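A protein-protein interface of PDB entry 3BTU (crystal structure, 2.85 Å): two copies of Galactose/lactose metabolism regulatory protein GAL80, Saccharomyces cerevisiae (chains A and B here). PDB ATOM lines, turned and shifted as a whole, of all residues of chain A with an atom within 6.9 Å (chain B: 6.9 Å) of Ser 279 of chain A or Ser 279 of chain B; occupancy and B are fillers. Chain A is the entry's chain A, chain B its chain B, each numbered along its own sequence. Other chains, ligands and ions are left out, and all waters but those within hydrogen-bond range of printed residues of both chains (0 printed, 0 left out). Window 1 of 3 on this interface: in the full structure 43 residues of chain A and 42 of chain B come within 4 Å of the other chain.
Of the printed residues of chain B, Ser 279 of chain A touches Ser 279 (3.3 Å), Cys 280 (3.9 Å) and Ser 281 (3.9 Å). Ser 279 of chain B touches three residues of chain A. Printed residues of chain A within 4 Å of Pro 277 of chain B: His 264 and Leu 266. Of the printed residues of chain A, Val 278 of chain B touches Leu 266 (3.8 Å). Printed residues of chain B within 4 Å of Leu 266 of chain A: Gln 268 (3.2 Å), Gly 269 (3.7 Å), Pro 277 (3.7 Å) and Val 278 (3.8 Å). Val 276 of chain A touches none of the printed residues of chain B. The nearest residue of chain B that does not touch Ser 279 of chain A is Leu 266 of chain B (4.3 Å). The nearest residue of chain A that does not touch Ser 279 of chain B is Leu 266 of chain A (4.2 Å).
The side-chain amide oxygen (OE1) of Gln 268 of chain A lies close to the side-chain amide oxygen (OE1) of Gln 268 of chain B. OG of Ser 281 of chain A lies within hydrogen-bond range of OE2 of Glu 180 of chain B (3.3 Å). NE2 of Gln 268 of chain B sits close to O of Leu 266 of chain A (3.4 Å). O of Phe 267 of chain B sits at hydrogen-bond distance from NE2 of Gln 268 of chain A (2.9 Å). The side-chain carboxylate (OE2) of Glu 180 of chain A sits at hydrogen-bond distance from the side-chain hydroxyl (OG) of Ser 281 of chain B (3.3 Å). The side-chain amide nitrogen of Gln 268 of chain A lies close to the backbone carbonyl oxygen of Leu 266 of chain B, at 3.5 Å. The side-chain hydroxyl of Ser 279 of chain B sits at hydrogen-bond distance from the side-chain hydroxyl of Ser 279 of chain A (3.3 Å). O of Phe 267 of chain A is in hydrogen-bond range of NE2 of Gln 268 of chain B, at 2.9 Å.
Ser 178 of chain A touches His 264 of chain B, and with the chains exchanged His 264 of chain A touches Ser 178 of chain B. Leu 266 of chain A touches Gly 269 of chain B, and with the chains exchanged Gly 269 of chain A touches Leu 266 of chain B. Leu 266 of chain A touches Pro 277 of chain B, and with the chains exchanged Pro 277 of chain A touches Leu 266 of chain B. Ser 279 of chain A touches Cys 280 of chain B, and with the chains exchanged Cys 280 of chain A touches Ser 279 of chain B. Positions printed for both chains: 178, 179, 180, 181, 182, 264, 265, 266, 267, 268, 269, 276, 277, 278, 279, 280 and 281. Of the 22 pairs that touch across the chains among the printed residues, 22 have their exchanged pair printed and touching as well.
O of Ile 181 of chain A lies within hydrogen-bond range of N of Ser 281 of chain A (3.1 Å). The backbone NH (N) of Ser 279 of chain A is in hydrogen-bond range of the backbone carbonyl oxygen (O) of Ile 179 of chain A, at 2.9 Å. A ring nitrogen (NE2) of His 264 of chain A lies within hydrogen-bond range of the side-chain hydroxyl (OG) of Ser 281 of chain A. The backbone carbonyl oxygen of Pro 277 of chain A lies within hydrogen-bond range of the backbone NH of Ile 179 of chain A (3.1 Å). The backbone NH (N) of Ile 179 of chain B lies within hydrogen-bond range of the backbone carbonyl oxygen (O) of Pro 277 of chain B. The backbone carbonyl oxygen of Gly 269 of chain A is in hydrogen-bond range of the backbone NH of Val 278 of chain A (2.9 Å).
Printed residues of chain B that touch a printed residue of chain A: Ser 178, Glu 180, His 264, Leu 266, Phe 267, Gln 268, Gly 269, Pro 277, Val 278, Ser 279, Cys 280 and Ser 281. Hydrophobic or aromatic side chains of chain B within 4 Å of the printed part of chain A: His 264, Leu 266 and Pro 277. Printed residues of chain A that touch a printed residue of chain B: Ser 178, Glu 180, His 264, Leu 266, Phe 267, Gln 268, Gly 269, Pro 277, Val 278, Ser 279, Cys 280 and Ser 281.
Among the printed residues, merely in contact across the chains: Ser 178 of chain A with His 264 of chain B (3.4 Å), His 264 of chain A with Ser 178 of chain B (3.4 Å), Gly 269 of chain A with Leu 266 of chain B (3.6 Å), Pro 277 of chain A with Leu 266 of chain B (3.6 Å), Leu 266 of chain A with Pro 277 of chain B (3.7 Å), Pro 277 of chain A with His 264 of chain B (3.7 Å), Leu 266 of chain A with Gly 269 of chain B (3.7 Å), His 264 of chain A with Pro 277 of chain B (3.7 Å), Leu 266 of chain A with Val 278 of chain B (3.8 Å), Val 278 of chain A with Leu 266 of chain B (3.8 Å), Ser 279 of chain A with Ser 281 of chain B (3.9 Å), Ser 279 of chain A with Cys 280 of chain B (3.9 Å), Cys 280 of chain A with Ser 279 of chain B (3.9 Å) and Ser 281 of chain A with Ser 279 of chain B (3.9 Å).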
ATOM      1  N   SER A 178     -17.627  22.026  21.162  1.00  0.00           N
ATOM      2  CA  SER A 178     -16.519  22.041  20.213  1.00  0.00           C
ATOM      3  C   SER A 178     -16.868  21.244  18.956  1.00  0.00           C
ATOM      4  O   SER A 178     -17.875  20.559  18.937  1.00  0.00           O
ATOM      5  CB  SER A 178     -15.243  21.504  20.859  1.00  0.00           C
ATOM      6  OG  SER A 178     -15.379  20.138  21.207  1.00  0.00           O
ATOM      7  N   ILE A 179     -16.037  21.337  17.918  1.00  0.00           N
ATOM      8  CA  ILE A 179     -16.341  20.740  16.614  1.00  0.00           C
ATOM      9  C   ILE A 179     -15.083  20.309  15.841  1.00  0.00           C
ATOM     10  O   ILE A 179     -14.120  21.068  15.742  1.00  0.00           O
ATOM     11  CB  ILE A 179     -17.107  21.728  15.733  1.00  0.00           C
ATOM     12  CG1 ILE A 179     -18.440  22.124  16.371  1.00  0.00           C
ATOM     13  CG2 ILE A 179     -17.316  21.142  14.332  1.00  0.00           C
ATOM     14  CD1 ILE A 179     -19.219  23.163  15.563  1.00  0.00           C
ATOM     15  N   GLU A 180     -15.086  19.105  15.281  1.00  0.00           N
ATOM     16  CA  GLU A 180     -13.990  18.677  14.417  1.00  0.00           C
ATOM     17  C   GLU A 180     -14.512  18.299  13.038  1.00  0.00           C
ATOM     18  O   GLU A 180     -15.605  17.765  12.918  1.00  0.00           O
ATOM     19  CB  GLU A 180     -13.240  17.495  15.019  1.00  0.00           C
ATOM     20  CG  GLU A 180     -12.493  17.812  16.300  1.00  0.00           C
ATOM     21  CD  GLU A 180     -13.324  17.552  17.561  1.00  0.00           C
ATOM     22  OE1 GLU A 180     -13.853  16.414  17.704  1.00  0.00           O
ATOM     23  OE2 GLU A 180     -13.431  18.482  18.412  1.00  0.00           O
ATOM     24  N   ILE A 181     -13.729  18.580  11.999  1.00  0.00           N
ATOM     25  CA  ILE A 181     -14.109  18.273  10.619  1.00  0.00           C
ATOM     26  C   ILE A 181     -12.944  17.663   9.837  1.00  0.00           C
ATOM     27  O   ILE A 181     -11.782  17.993  10.074  1.00  0.00           O
ATOM     28  CB  ILE A 181     -14.571  19.520   9.869  1.00  0.00           C
ATOM     29  CG1 ILE A 181     -15.837  20.095  10.495  1.00  0.00           C
ATOM     30  CG2 ILE A 181     -14.819  19.202   8.405  1.00  0.00           C
ATOM     31  CD1 ILE A 181     -16.454  21.195   9.655  1.00  0.00           C
ATOM     32  N   ALA A 182     -13.259  16.764   8.911  1.00  0.00           N
ATOM     33  CA  ALA A 182     -12.246  16.145   8.069  1.00  0.00           C
ATOM     34  C   ALA A 182     -12.829  15.831   6.693  1.00  0.00           C
ATOM     35  O   ALA A 182     -13.925  15.267   6.578  1.00  0.00           O
ATOM     36  CB  ALA A 182     -11.718  14.885   8.723  1.00  0.00           C
ATOM     37  N   HIS A 264      -3.376  20.018   0.626  1.00  0.00           N
ATOM     38  CA  HIS A 264      -3.797  19.850   2.011  1.00  0.00           C
ATOM     39  C   HIS A 264      -4.145  21.187   2.644  1.00  0.00           C
ATOM     40  O   HIS A 264      -3.473  22.192   2.414  1.00  0.00           O
ATOM     41  CB  HIS A 264      -2.754  19.124   2.865  1.00  0.00           C
ATOM     42  CG  HIS A 264      -3.319  18.579   4.139  1.00  0.00           C
ATOM     43  ND1 HIS A 264      -3.591  17.233   4.329  1.00  0.00           N
ATOM     44  CD2 HIS A 264      -3.725  19.195   5.275  1.00  0.00           C
ATOM     45  CE1 HIS A 264      -4.113  17.054   5.526  1.00  0.00           C
ATOM     46  NE2 HIS A 264      -4.213  18.228   6.121  1.00  0.00           N
ATOM     47  N   LEU A 265      -5.204  21.198   3.441  1.00  0.00           N
ATOM     48  CA  LEU A 265      -5.613  22.406   4.130  1.00  0.00           C
ATOM     49  C   LEU A 265      -5.759  22.143   5.626  1.00  0.00           C
ATOM     50  O   LEU A 265      -6.510  21.263   6.018  1.00  0.00           O
ATOM     51  CB  LEU A 265      -6.945  22.904   3.576  1.00  0.00           C
ATOM     52  CG  LEU A 265      -7.634  23.932   4.471  1.00  0.00           C
ATOM     53  CD1 LEU A 265      -6.878  25.243   4.398  1.00  0.00           C
ATOM     54  CD2 LEU A 265      -9.100  24.135   4.115  1.00  0.00           C
ATOM     55  N   LEU A 266      -5.040  22.895   6.456  1.00  0.00           N
ATOM     56  CA  LEU A 266      -5.269  22.899   7.896  1.00  0.00           C
ATOM     57  C   LEU A 266      -6.051  24.155   8.217  1.00  0.00           C
ATOM     58  O   LEU A 266      -5.521  25.241   8.081  1.00  0.00           O
ATOM     59  CB  LEU A 266      -3.937  22.955   8.642  1.00  0.00           C
ATOM     60  CG  LEU A 266      -3.319  21.680   9.223  1.00  0.00           C
ATOM     61  CD1 LEU A 266      -3.841  20.381   8.569  1.00  0.00           C
ATOM     62  CD2 LEU A 266      -1.798  21.768   9.144  1.00  0.00           C
ATOM     63  N   PHE A 267      -7.308  24.030   8.621  1.00  0.00           N
ATOM     64  CA  PHE A 267      -8.093  25.209   8.987  1.00  0.00           C
ATOM     65  C   PHE A 267      -8.468  25.096  10.452  1.00  0.00           C
ATOM     66  O   PHE A 267      -8.439  24.007  11.011  1.00  0.00           O
ATOM     67  CB  PHE A 267      -9.335  25.333   8.107  1.00  0.00           C
ATOM     68  CG  PHE A 267     -10.336  26.336   8.595  1.00  0.00           C
ATOM     69  CD1 PHE A 267     -10.308  27.634   8.140  1.00  0.00           C
ATOM     70  CD2 PHE A 267     -11.321  25.973   9.491  1.00  0.00           C
ATOM     71  CE1 PHE A 267     -11.237  28.556   8.581  1.00  0.00           C
ATOM     72  CE2 PHE A 267     -12.259  26.890   9.929  1.00  0.00           C
ATOM     73  CZ  PHE A 267     -12.218  28.179   9.476  1.00  0.00           C
ATOM     74  N   GLN A 268      -8.829  26.209  11.078  1.00  0.00           N
ATOM     75  CA  GLN A 268      -8.919  26.241  12.529  1.00  0.00           C
ATOM     76  C   GLN A 268      -9.437  27.593  12.962  1.00  0.00           C
ATOM     77  O   GLN A 268      -8.821  28.612  12.666  1.00  0.00           O
ATOM     78  CB  GLN A 268      -7.514  26.038  13.086  1.00  0.00           C
ATOM     79  CG  GLN A 268      -7.411  25.902  14.576  1.00  0.00           C
ATOM     80  CD  GLN A 268      -5.982  25.616  15.008  1.00  0.00           C
ATOM     81  OE1 GLN A 268      -5.111  26.483  14.921  1.00  0.00           O
ATOM     82  NE2 GLN A 268      -5.734  24.395  15.475  1.00  0.00           N
ATOM     83  N   GLY A 269     -10.559  27.626  13.659  1.00  0.00           N
ATOM     84  CA  GLY A 269     -11.128  28.908  14.012  1.00  0.00           C
ATOM     85  C   GLY A 269     -12.223  28.827  15.046  1.00  0.00           C
ATOM     86  O   GLY A 269     -12.304  27.852  15.790  1.00  0.00           O
ATOM     87  N   VAL A 276     -17.168  28.921  19.724  1.00  0.00           N
ATOM     88  CA  VAL A 276     -16.975  27.479  19.614  1.00  0.00           C
ATOM     89  C   VAL A 276     -15.734  27.103  18.818  1.00  0.00           C
ATOM     90  O   VAL A 276     -15.625  27.449  17.645  1.00  0.00           O
ATOM     91  CB  VAL A 276     -18.157  26.854  18.875  1.00  0.00           C
ATOM     92  CG1 VAL A 276     -17.973  25.350  18.790  1.00  0.00           C
ATOM     93  CG2 VAL A 276     -19.462  27.225  19.562  1.00  0.00           C
ATOM     94  N   PRO A 277     -14.804  26.367  19.438  1.00  0.00           N
ATOM     95  CA  PRO A 277     -13.603  25.963  18.698  1.00  0.00           C
ATOM     96  C   PRO A 277     -13.979  25.063  17.537  1.00  0.00           C
ATOM     97  O   PRO A 277     -14.860  24.220  17.703  1.00  0.00           O
ATOM     98  CB  PRO A 277     -12.812  25.152  19.724  1.00  0.00           C
ATOM     99  CG  PRO A 277     -13.330  25.593  21.039  1.00  0.00           C
ATOM    100  CD  PRO A 277     -14.775  25.914  20.833  1.00  0.00           C
ATOM    101  N   VAL A 278     -13.334  25.239  16.386  1.00  0.00           N
ATOM    102  CA  VAL A 278     -13.540  24.344  15.252  1.00  0.00           C
ATOM    103  C   VAL A 278     -12.185  23.919  14.729  1.00  0.00           C
ATOM    104  O   VAL A 278     -11.350  24.769  14.443  1.00  0.00           O
ATOM    105  CB  VAL A 278     -14.299  25.042  14.107  1.00  0.00           C
ATOM    106  CG1 VAL A 278     -14.387  24.124  12.905  1.00  0.00           C
ATOM    107  CG2 VAL A 278     -15.687  25.465  14.557  1.00  0.00           C
ATOM    108  N   SER A 279     -11.957  22.617  14.611  1.00  0.00           N
ATOM    109  CA  SER A 279     -10.692  22.120  14.082  1.00  0.00           C
ATOM    110  C   SER A 279     -10.920  21.456  12.727  1.00  0.00           C
ATOM    111  O   SER A 279     -11.876  20.711  12.575  1.00  0.00           O
ATOM    112  CB  SER A 279     -10.058  21.128  15.067  1.00  0.00           C
ATOM    113  OG  SER A 279      -9.204  20.205  14.399  1.00  0.00           O
ATOM    114  N   CYS A 280     -10.064  21.714  11.741  1.00  0.00           N
ATOM    115  CA  CYS A 280     -10.283  21.142  10.413  1.00  0.00           C
ATOM    116  C   CYS A 280      -9.036  20.574   9.770  1.00  0.00           C
ATOM    117  O   CYS A 280      -7.948  21.113   9.911  1.00  0.00           O
ATOM    118  CB  CYS A 280     -10.898  22.175   9.479  1.00  0.00           C
ATOM    119  SG  CYS A 280     -12.652  22.457   9.774  1.00  0.00           S
ATOM    120  N   SER A 281      -9.211  19.480   9.045  1.00  0.00           N
ATOM    121  CA  SER A 281      -8.139  18.906   8.251  1.00  0.00           C
ATOM    122  C   SER A 281      -8.705  18.372   6.933  1.00  0.00           C
ATOM    123  O   SER A 281      -9.568  17.499   6.947  1.00  0.00           O
ATOM    124  CB  SER A 281      -7.460  17.791   9.038  1.00  0.00           C
ATOM    125  OG  SER A 281      -6.225  17.425   8.448  1.00  0.00           O
ATOM    126  N   SER B 178      -0.091  13.036   6.321  1.00  0.00           N
ATOM    127  CA  SER B 178      -0.750  13.978   7.219  1.00  0.00           C
ATOM    128  C   SER B 178      -1.097  13.325   8.558  1.00  0.00           C
ATOM    129  O   SER B 178      -0.988  12.110   8.700  1.00  0.00           O
ATOM    130  CB  SER B 178      -1.993  14.571   6.553  1.00  0.00           C
ATOM    131  OG  SER B 178      -2.987  13.591   6.324  1.00  0.00           O
ATOM    132  N   ILE B 179      -1.522  14.114   9.539  1.00  0.00           N
ATOM    133  CA  ILE B 179      -1.755  13.573  10.882  1.00  0.00           C
ATOM    134  C   ILE B 179      -2.872  14.311  11.632  1.00  0.00           C
ATOM    135  O   ILE B 179      -2.914  15.534  11.626  1.00  0.00           O
ATOM    136  CB  ILE B 179      -0.478  13.661  11.734  1.00  0.00           C
ATOM    137  CG1 ILE B 179       0.645  12.815  11.141  1.00  0.00           C
ATOM    138  CG2 ILE B 179      -0.752  13.216  13.155  1.00  0.00           C
ATOM    139  CD1 ILE B 179       1.944  12.894  11.935  1.00  0.00           C
ATOM    140  N   GLU B 180      -3.765  13.587  12.297  1.00  0.00           N
ATOM    141  CA  GLU B 180      -4.758  14.247  13.137  1.00  0.00           C
ATOM    142  C   GLU B 180      -4.675  13.724  14.562  1.00  0.00           C
ATOM    143  O   GLU B 180      -4.382  12.560  14.774  1.00  0.00           O
ATOM    144  CB  GLU B 180      -6.173  14.050  12.593  1.00  0.00           C
ATOM    145  CG  GLU B 180      -6.454  14.744  11.266  1.00  0.00           C
ATOM    146  CD  GLU B 180      -6.183  13.852  10.066  1.00  0.00           C
ATOM    147  OE1 GLU B 180      -6.765  12.741  10.003  1.00  0.00           O
ATOM    148  OE2 GLU B 180      -5.392  14.270   9.182  1.00  0.00           O
ATOM    149  N   ILE B 181      -4.931  14.585  15.540  1.00  0.00           N
ATOM    150  CA  ILE B 181      -4.886  14.197  16.944  1.00  0.00           C
ATOM    151  C   ILE B 181      -6.080  14.761  17.714  1.00  0.00           C
ATOM    152  O   ILE B 181      -6.578  15.837  17.399  1.00  0.00           O
ATOM    153  CB  ILE B 181      -3.599  14.698  17.618  1.00  0.00           C
ATOM    154  CG1 ILE B 181      -2.365  14.053  16.985  1.00  0.00           C
ATOM    155  CG2 ILE B 181      -3.633  14.408  19.103  1.00  0.00           C
ATOM    156  CD1 ILE B 181      -1.095  14.286  17.773  1.00  0.00           C
ATOM    157  N   ALA B 182      -6.536  14.036  18.726  1.00  0.00           N
ATOM    158  CA  ALA B 182      -7.622  14.507  19.567  1.00  0.00           C
ATOM    159  C   ALA B 182      -7.448  13.952  20.979  1.00  0.00           C
ATOM    160  O   ALA B 182      -7.235  12.748  21.151  1.00  0.00           O
ATOM    161  CB  ALA B 182      -8.961  14.087  18.990  1.00  0.00           C
ATOM    162  N   HIS B 264      -9.947  24.328  26.413  1.00  0.00           N
ATOM    163  CA  HIS B 264      -9.854  23.794  25.066  1.00  0.00           C
ATOM    164  C   HIS B 264      -8.628  24.324  24.353  1.00  0.00           C
ATOM    165  O   HIS B 264      -8.265  25.489  24.508  1.00  0.00           O
ATOM    166  CB  HIS B 264     -11.106  24.088  24.235  1.00  0.00           C
ATOM    167  CG  HIS B 264     -11.216  23.228  23.015  1.00  0.00           C
ATOM    168  ND1 HIS B 264     -12.083  22.160  22.939  1.00  0.00           N
ATOM    169  CD2 HIS B 264     -10.529  23.241  21.853  1.00  0.00           C
ATOM    170  CE1 HIS B 264     -11.951  21.572  21.763  1.00  0.00           C
ATOM    171  NE2 HIS B 264     -11.012  22.211  21.083  1.00  0.00           N
ATOM    172  N   LEU B 265      -7.994  23.462  23.568  1.00  0.00           N
ATOM    173  CA  LEU B 265      -6.819  23.840  22.799  1.00  0.00           C
ATOM    174  C   LEU B 265      -6.996  23.433  21.352  1.00  0.00           C
ATOM    175  O   LEU B 265      -7.247  22.271  21.074  1.00  0.00           O
ATOM    176  CB  LEU B 265      -5.569  23.159  23.349  1.00  0.00           C
ATOM    177  CG  LEU B 265      -4.373  23.207  22.398  1.00  0.00           C
ATOM    178  CD1 LEU B 265      -3.810  24.606  22.364  1.00  0.00           C
ATOM    179  CD2 LEU B 265      -3.286  22.223  22.797  1.00  0.00           C
ATOM    180  N   LEU B 266      -6.873  24.390  20.435  1.00  0.00           N
ATOM    181  CA  LEU B 266      -6.773  24.102  19.000  1.00  0.00           C
ATOM    182  C   LEU B 266      -5.312  24.266  18.629  1.00  0.00           C
ATOM    183  O   LEU B 266      -4.791  25.375  18.672  1.00  0.00           O
ATOM    184  CB  LEU B 266      -7.590  25.115  18.209  1.00  0.00           C
ATOM    185  CG  LEU B 266      -8.995  24.770  17.731  1.00  0.00           C
ATOM    186  CD1 LEU B 266      -9.627  23.643  18.507  1.00  0.00           C
ATOM    187  CD2 LEU B 266      -9.869  26.010  17.766  1.00  0.00           C
ATOM    188  N   PHE B 267      -4.626  23.183  18.296  1.00  0.00           N
ATOM    189  CA  PHE B 267      -3.233  23.307  17.872  1.00  0.00           C
ATOM    190  C   PHE B 267      -3.117  22.849  16.432  1.00  0.00           C
ATOM    191  O   PHE B 267      -3.986  22.127  15.952  1.00  0.00           O
ATOM    192  CB  PHE B 267      -2.321  22.494  18.774  1.00  0.00           C
ATOM    193  CG  PHE B 267      -0.930  22.312  18.243  1.00  0.00           C
ATOM    194  CD1 PHE B 267       0.073  23.192  18.585  1.00  0.00           C
ATOM    195  CD2 PHE B 267      -0.615  21.233  17.443  1.00  0.00           C
ATOM    196  CE1 PHE B 267       1.368  23.015  18.124  1.00  0.00           C
ATOM    197  CE2 PHE B 267       0.675  21.044  16.979  1.00  0.00           C
ATOM    198  CZ  PHE B 267       1.670  21.939  17.323  1.00  0.00           C
ATOM    199  N   GLN B 268      -2.056  23.251  15.743  1.00  0.00           N
ATOM    200  CA  GLN B 268      -2.021  23.095  14.299  1.00  0.00           C
ATOM    201  C   GLN B 268      -0.650  23.498  13.798  1.00  0.00           C
ATOM    202  O   GLN B 268      -0.225  24.624  14.014  1.00  0.00           O
ATOM    203  CB  GLN B 268      -3.078  24.017  13.707  1.00  0.00           C
ATOM    204  CG  GLN B 268      -3.313  23.868  12.242  1.00  0.00           C
ATOM    205  CD  GLN B 268      -4.418  24.787  11.762  1.00  0.00           C
ATOM    206  OE1 GLN B 268      -4.264  26.006  11.777  1.00  0.00           O
ATOM    207  NE2 GLN B 268      -5.541  24.206  11.326  1.00  0.00           N
ATOM    208  N   GLY B 269       0.061  22.596  13.140  1.00  0.00           N
ATOM    209  CA  GLY B 269       1.410  22.925  12.725  1.00  0.00           C
ATOM    210  C   GLY B 269       2.003  21.967  11.727  1.00  0.00           C
ATOM    211  O   GLY B 269       1.282  21.230  11.053  1.00  0.00           O
ATOM    212  N   VAL B 276       5.010  17.802   7.247  1.00  0.00           N
ATOM    213  CA  VAL B 276       3.778  17.049   7.454  1.00  0.00           C
ATOM    214  C   VAL B 276       2.722  17.834   8.211  1.00  0.00           C
ATOM    215  O   VAL B 276       2.949  18.237   9.339  1.00  0.00           O
ATOM    216  CB  VAL B 276       4.063  15.819   8.293  1.00  0.00           C
ATOM    217  CG1 VAL B 276       2.800  15.017   8.477  1.00  0.00           C
ATOM    218  CG2 VAL B 276       5.149  14.984   7.652  1.00  0.00           C
ATOM    219  N   PRO B 277       1.551  18.047   7.602  1.00  0.00           N
ATOM    220  CA  PRO B 277       0.510  18.788   8.324  1.00  0.00           C
ATOM    221  C   PRO B 277       0.091  18.032   9.574  1.00  0.00           C
ATOM    222  O   PRO B 277       0.001  16.808   9.515  1.00  0.00           O
ATOM    223  CB  PRO B 277      -0.662  18.811   7.323  1.00  0.00           C
ATOM    224  CG  PRO B 277      -0.040  18.600   6.004  1.00  0.00           C
ATOM    225  CD  PRO B 277       1.148  17.717   6.228  1.00  0.00           C
ATOM    226  N   VAL B 278      -0.158  18.727  10.677  1.00  0.00           N
ATOM    227  CA  VAL B 278      -0.683  18.082  11.878  1.00  0.00           C
ATOM    228  C   VAL B 278      -1.829  18.920  12.386  1.00  0.00           C
ATOM    229  O   VAL B 278      -1.682  20.134  12.554  1.00  0.00           O
ATOM    230  CB  VAL B 278       0.369  18.017  12.984  1.00  0.00           C
ATOM    231  CG1 VAL B 278      -0.249  17.466  14.250  1.00  0.00           C
ATOM    232  CG2 VAL B 278       1.566  17.178  12.547  1.00  0.00           C
ATOM    233  N   SER B 279      -2.971  18.295  12.624  1.00  0.00           N
ATOM    234  CA  SER B 279      -4.138  19.017  13.128  1.00  0.00           C
ATOM    235  C   SER B 279      -4.454  18.529  14.536  1.00  0.00           C
ATOM    236  O   SER B 279      -4.438  17.337  14.779  1.00  0.00           O
ATOM    237  CB  SER B 279      -5.346  18.810  12.198  1.00  0.00           C
ATOM    238  OG  SER B 279      -6.590  18.954  12.879  1.00  0.00           O
ATOM    239  N   CYS B 280      -4.753  19.428  15.466  1.00  0.00           N
ATOM    240  CA  CYS B 280      -5.038  18.994  16.826  1.00  0.00           C
ATOM    241  C   CYS B 280      -6.255  19.644  17.449  1.00  0.00           C
ATOM    242  O   CYS B 280      -6.545  20.805  17.194  1.00  0.00           O
ATOM    243  CB  CYS B 280      -3.826  19.233  17.716  1.00  0.00           C
ATOM    244  SG  CYS B 280      -2.506  18.031  17.458  1.00  0.00           S
ATOM    245  N   SER B 281      -6.959  18.884  18.279  1.00  0.00           N
ATOM    246  CA  SER B 281      -8.067  19.413  19.056  1.00  0.00           C
ATOM    247  C   SER B 281      -8.104  18.740  20.422  1.00  0.00           C
ATOM    248  O   SER B 281      -8.268  17.523  20.508  1.00  0.00           O
ATOM    249  CB  SER B 281      -9.383  19.169  18.319  1.00  0.00           C
ATOM    250  OG  SER B 281     -10.459  19.867  18.928  1.00  0.00           O
